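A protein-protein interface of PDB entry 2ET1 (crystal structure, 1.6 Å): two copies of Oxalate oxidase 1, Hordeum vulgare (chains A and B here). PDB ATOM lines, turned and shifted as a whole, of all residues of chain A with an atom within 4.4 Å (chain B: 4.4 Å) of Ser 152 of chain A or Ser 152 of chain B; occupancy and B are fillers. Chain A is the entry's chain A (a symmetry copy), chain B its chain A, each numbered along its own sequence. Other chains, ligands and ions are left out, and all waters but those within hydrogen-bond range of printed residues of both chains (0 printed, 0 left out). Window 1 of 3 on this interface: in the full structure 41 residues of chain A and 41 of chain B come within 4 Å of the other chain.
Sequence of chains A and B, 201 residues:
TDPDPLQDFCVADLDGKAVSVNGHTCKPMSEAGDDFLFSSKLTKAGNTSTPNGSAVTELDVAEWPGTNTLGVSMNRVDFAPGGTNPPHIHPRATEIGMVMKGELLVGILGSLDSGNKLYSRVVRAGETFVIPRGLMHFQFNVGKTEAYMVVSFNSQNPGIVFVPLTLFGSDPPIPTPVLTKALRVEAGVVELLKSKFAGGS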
ATOM      1  N   SER A  73     -14.678   2.460 -22.076  1.00  0.00           N
ATOM      2  CA  SER A  73     -14.458   3.040 -20.729  1.00  0.00           C
ATOM      3  C   SER A  73     -12.990   2.837 -20.327  1.00  0.00           C
ATOM      4  O   SER A  73     -12.244   2.154 -21.034  1.00  0.00           O
ATOM      5  CB  SER A  73     -15.395   2.409 -19.682  1.00  0.00           C
ATOM      6  OG  SER A  73     -15.088   1.041 -19.449  1.00  0.00           O
ATOM      7  N   MET A  74     -12.585   3.441 -19.206  1.00  0.00           N
ATOM      8  CA  MET A  74     -11.184   3.375 -18.719  1.00  0.00           C
ATOM      9  C   MET A  74     -11.152   3.330 -17.198  1.00  0.00           C
ATOM     10  O   MET A  74     -11.970   3.987 -16.558  1.00  0.00           O
ATOM     11  CB  MET A  74     -10.441   4.655 -19.108  1.00  0.00           C
ATOM     12  CG  MET A  74      -9.647   4.666 -20.360  1.00  0.00           C
ATOM     13  SD  MET A  74      -8.849   6.300 -20.450  1.00  0.00           S
ATOM     14  CE  MET A  74      -7.675   6.233 -19.171  1.00  0.00           C
ATOM     15  N   THR A  94     -13.239  -7.173 -23.304  1.00  0.00           N
ATOM     16  CA  THR A  94     -11.766  -7.267 -23.395  1.00  0.00           C
ATOM     17  C   THR A  94     -11.140  -6.017 -22.766  1.00  0.00           C
ATOM     18  O   THR A  94     -11.707  -4.924 -22.851  1.00  0.00           O
ATOM     19  CB  THR A  94     -11.318  -7.359 -24.882  1.00  0.00           C
ATOM     20  OG1 THR A  94     -11.836  -8.559 -25.486  1.00  0.00           O
ATOM     21  CG2 THR A  94      -9.770  -7.392 -25.025  1.00  0.00           C
ATOM     22  N   GLU A  95      -9.957  -6.188 -22.160  1.00  0.00           N
ATOM     23  CA  GLU A  95      -9.165  -5.097 -21.559  1.00  0.00           C
ATOM     24  C   GLU A  95      -7.836  -4.922 -22.301  1.00  0.00           C
ATOM     25  O   GLU A  95      -7.212  -5.911 -22.721  1.00  0.00           O
ATOM     26  CB  GLU A  95      -8.882  -5.438 -20.087  1.00  0.00           C
ATOM     27  CG  GLU A  95      -7.989  -4.438 -19.332  1.00  0.00           C
ATOM     28  CD  GLU A  95      -7.728  -4.866 -17.894  1.00  0.00           C
ATOM     29  OE1 GLU A  95      -8.606  -5.528 -17.298  1.00  0.00           O
ATOM     30  OE2 GLU A  95      -6.630  -4.548 -17.363  1.00  0.00           O
ATOM     31  N   ILE A  96      -7.413  -3.666 -22.463  1.00  0.00           N
ATOM     32  CA  ILE A  96      -6.099  -3.347 -23.037  1.00  0.00           C
ATOM     33  C   ILE A  96      -5.430  -2.312 -22.130  1.00  0.00           C
ATOM     34  O   ILE A  96      -5.998  -1.247 -21.858  1.00  0.00           O
ATOM     35  CB  ILE A  96      -6.218  -2.908 -24.534  1.00  0.00           C
ATOM     36  CG1 ILE A  96      -4.849  -2.801 -25.202  1.00  0.00           C
ATOM     37  CG2 ILE A  96      -7.056  -1.610 -24.705  1.00  0.00           C
ATOM     38  CD1 ILE A  96      -4.933  -2.831 -26.756  1.00  0.00           C
ATOM     39  N   VAL A 151      -6.000   1.377 -17.881  1.00  0.00           N
ATOM     40  CA  VAL A 151      -6.532   0.292 -18.723  1.00  0.00           C
ATOM     41  C   VAL A 151      -7.833   0.738 -19.381  1.00  0.00           C
ATOM     42  O   VAL A 151      -8.590   1.506 -18.785  1.00  0.00           O
ATOM     43  CB  VAL A 151      -6.751  -1.021 -17.919  1.00  0.00           C
ATOM     44  CG1 VAL A 151      -5.438  -1.465 -17.289  1.00  0.00           C
ATOM     45  CG2 VAL A 151      -7.789  -0.856 -16.828  1.00  0.00           C
ATOM     46  N   SER A 152      -8.066   0.271 -20.609  1.00  0.00           N
ATOM     47  CA  SER A 152      -9.268   0.627 -21.369  1.00  0.00           C
ATOM     48  C   SER A 152     -10.055  -0.648 -21.693  1.00  0.00           C
ATOM     49  O   SER A 152      -9.475  -1.744 -21.731  1.00  0.00           O
ATOM     50  CB  SER A 152      -8.878   1.342 -22.672  1.00  0.00           C
ATOM     51  OG  SER A 152      -8.175   2.556 -22.406  1.00  0.00           O
ATOM     52  N   PHE A 153     -11.355  -0.497 -21.944  1.00  0.00           N
ATOM     53  CA  PHE A 153     -12.245  -1.642 -22.204  1.00  0.00           C
ATOM     54  C   PHE A 153     -13.110  -1.386 -23.425  1.00  0.00           C
ATOM     55  O   PHE A 153     -13.483  -0.234 -23.682  1.00  0.00           O
ATOM     56  CB  PHE A 153     -13.194  -1.887 -21.015  1.00  0.00           C
ATOM     57  CG  PHE A 153     -12.493  -2.094 -19.691  1.00  0.00           C
ATOM     58  CD1 PHE A 153     -12.255  -1.009 -18.841  1.00  0.00           C
ATOM     59  CD2 PHE A 153     -12.103  -3.373 -19.286  1.00  0.00           C
ATOM     60  CE1 PHE A 153     -11.594  -1.192 -17.615  1.00  0.00           C
ATOM     61  CE2 PHE A 153     -11.430  -3.577 -18.066  1.00  0.00           C
ATOM     62  CZ  PHE A 153     -11.186  -2.476 -17.223  1.00  0.00           C
ATOM     63  N   SER B  73      -7.334  -2.152 -29.768  1.00  0.00           N
ATOM     64  CA  SER B  73      -5.970  -1.752 -30.190  1.00  0.00           C
ATOM     65  C   SER B  73      -5.608  -0.418 -29.523  1.00  0.00           C
ATOM     66  O   SER B  73      -6.457   0.201 -28.877  1.00  0.00           O
ATOM     67  CB  SER B  73      -5.864  -1.634 -31.722  1.00  0.00           C
ATOM     68  OG  SER B  73      -6.638  -0.555 -32.228  1.00  0.00           O
ATOM     69  N   MET B  74      -4.350   0.007 -29.673  1.00  0.00           N
ATOM     70  CA  MET B  74      -3.841   1.253 -29.046  1.00  0.00           C
ATOM     71  C   MET B  74      -2.838   1.939 -29.962  1.00  0.00           C
ATOM     72  O   MET B  74      -2.065   1.254 -30.628  1.00  0.00           O
ATOM     73  CB  MET B  74      -3.068   0.912 -27.771  1.00  0.00           C
ATOM     74  CG  MET B  74      -3.781   0.951 -26.471  1.00  0.00           C
ATOM     75  SD  MET B  74      -2.541   0.577 -25.192  1.00  0.00           S
ATOM     76  CE  MET B  74      -1.534   1.993 -25.197  1.00  0.00           C
ATOM     77  N   THR B  94     -14.849   3.723 -32.087  1.00  0.00           N
ATOM     78  CA  THR B  94     -14.742   4.795 -31.074  1.00  0.00           C
ATOM     79  C   THR B  94     -13.318   4.813 -30.506  1.00  0.00           C
ATOM     80  O   THR B  94     -12.682   3.762 -30.381  1.00  0.00           O
ATOM     81  CB  THR B  94     -15.743   4.545 -29.910  1.00  0.00           C
ATOM     82  OG1 THR B  94     -17.097   4.587 -30.400  1.00  0.00           O
ATOM     83  CG2 THR B  94     -15.616   5.614 -28.788  1.00  0.00           C
ATOM     84  N   GLU B  95     -12.840   6.011 -30.143  1.00  0.00           N
ATOM     85  CA  GLU B  95     -11.523   6.224 -29.512  1.00  0.00           C
ATOM     86  C   GLU B  95     -11.687   6.770 -28.089  1.00  0.00           C
ATOM     87  O   GLU B  95     -12.580   7.592 -27.827  1.00  0.00           O
ATOM     88  CB  GLU B  95     -10.725   7.234 -30.353  1.00  0.00           C
ATOM     89  CG  GLU B  95      -9.352   7.635 -29.785  1.00  0.00           C
ATOM     90  CD  GLU B  95      -8.643   8.663 -30.656  1.00  0.00           C
ATOM     91  OE1 GLU B  95      -8.855   8.651 -31.888  1.00  0.00           O
ATOM     92  OE2 GLU B  95      -7.879   9.496 -30.100  1.00  0.00           O
ATOM     93  N   ILE B  96     -10.827   6.307 -27.179  1.00  0.00           N
ATOM     94  CA  ILE B  96     -10.776   6.832 -25.808  1.00  0.00           C
ATOM     95  C   ILE B  96      -9.311   7.117 -25.468  1.00  0.00           C
ATOM     96  O   ILE B  96      -8.454   6.230 -25.572  1.00  0.00           O
ATOM     97  CB  ILE B  96     -11.495   5.875 -24.800  1.00  0.00           C
ATOM     98  CG1 ILE B  96     -11.651   6.518 -23.424  1.00  0.00           C
ATOM     99  CG2 ILE B  96     -10.814   4.480 -24.721  1.00  0.00           C
ATOM    100  CD1 ILE B  96     -12.738   5.823 -22.554  1.00  0.00           C
ATOM    101  N   VAL B 151      -3.876   6.436 -26.876  1.00  0.00           N
ATOM    102  CA  VAL B 151      -5.311   6.305 -27.183  1.00  0.00           C
ATOM    103  C   VAL B 151      -5.645   4.848 -27.480  1.00  0.00           C
ATOM    104  O   VAL B 151      -4.812   4.127 -28.031  1.00  0.00           O
ATOM    105  CB  VAL B 151      -5.744   7.215 -28.368  1.00  0.00           C
ATOM    106  CG1 VAL B 151      -5.424   8.669 -28.045  1.00  0.00           C
ATOM    107  CG2 VAL B 151      -5.052   6.835 -29.660  1.00  0.00           C
ATOM    108  N   SER B 152      -6.850   4.426 -27.091  1.00  0.00           N
ATOM    109  CA  SER B 152      -7.302   3.046 -27.298  1.00  0.00           C
ATOM    110  C   SER B 152      -8.563   3.055 -28.169  1.00  0.00           C
ATOM    111  O   SER B 152      -9.283   4.065 -28.212  1.00  0.00           O
ATOM    112  CB  SER B 152      -7.610   2.382 -25.947  1.00  0.00           C
ATOM    113  OG  SER B 152      -6.445   2.323 -25.122  1.00  0.00           O
ATOM    114  N   PHE B 153      -8.834   1.933 -28.835  1.00  0.00           N
ATOM    115  CA  PHE B 153      -9.975   1.822 -29.761  1.00  0.00           C
ATOM    116  C   PHE B 153     -10.758   0.547 -29.502  1.00  0.00           C
ATOM    117  O   PHE B 153     -10.164  -0.469 -29.117  1.00  0.00           O
ATOM    118  CB  PHE B 153      -9.496   1.775 -31.225  1.00  0.00           C
ATOM    119  CG  PHE B 153      -8.636   2.948 -31.637  1.00  0.00           C
ATOM    120  CD1 PHE B 153      -7.243   2.872 -31.535  1.00  0.00           C
ATOM    121  CD2 PHE B 153      -9.216   4.110 -32.154  1.00  0.00           C
ATOM    122  CE1 PHE B 153      -6.437   3.961 -31.904  1.00  0.00           C
ATOM    123  CE2 PHE B 153      -8.428   5.218 -32.521  1.00  0.00           C
ATOM    124  CZ  PHE B 153      -7.028   5.132 -32.403  1.00  0.00           C
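Of the 8 printed residues of chain A, 4 touch a printed residue of chain B. Hydrophobic or aromatic side chains of chain A within 4 Å of the printed part of chain B: Met 74 and Ile 96. Of the 8 printed residues of chain B, 4 touch a printed residue of chain A. Among the printed residues, no Asp or Glu carboxylate lies within 4 Å of a Lys or Arg side-chain nitrogen of the other chain.
Among the printed residues, merely in contact across the chains: Ile 96 of chain A with Ser 73 of chain B, Ser 73 of chain A with Ile 96 of chain B, Met 74 of chain A with Ile 96 of chain B and Ile 96 of chain A with Met 74 of chain B.
Of the printed residues of chain B, Ser 152 of chain A touches Ser 152. Printed residues of chain A within 4 Å of Met 74 of chain B: Ile 96. Printed residues of chain B within 4 Å of Ser 73 of chain A: Ile 96 (3.7 Å). The nearest printed residue of chain B that does not touch Ser 152 of chain A is Ile 96 of chain B (4.003 Å). The nearest printed residue of chain B that does not touch Met 74 of chain A is Ser 152 of chain B (6.2 Å).
The backbone carbonyl oxygen (O) of Ser 73 of chain B lies within hydrogen-bond range of the backbone NH (N) of Phe 153 of chain B, at 2.9 Å. O of Ile 96 of chain A sits at hydrogen-bond distance from N of Ser 152 of chain A (2.9 Å). The backbone carbonyl oxygen (O) of Ile 96 of chain B lies within hydrogen-bond range of the backbone NH (N) of Ser 152 of chain B (2.9 Å). The backbone carbonyl oxygen (O) of Ser 73 of chain A lies within hydrogen-bond range of the backbone NH (N) of Phe 153 of chain A (2.9 Å).
Ser 73 of chain A touches Ile 96 of chain B, and with the chains exchanged Ile 96 of chain A touches Ser 73 of chain B. Met 74 of chain A touches Ile 96 of chain B, and with the chains exchanged Ile 96 of chain A touches Met 74 of chain B. Ser 152 of chain A touches its own counterpart, Ser 152 of chain B. Positions printed for both chains: 73, 74, 94, 95, 96, 151, 152 and 153.
The side-chain hydroxyl of Ser 152 of chain B lies within hydrogen-bond range of the side-chain hydroxyl of Ser 152 of chain A (3.2 Å).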
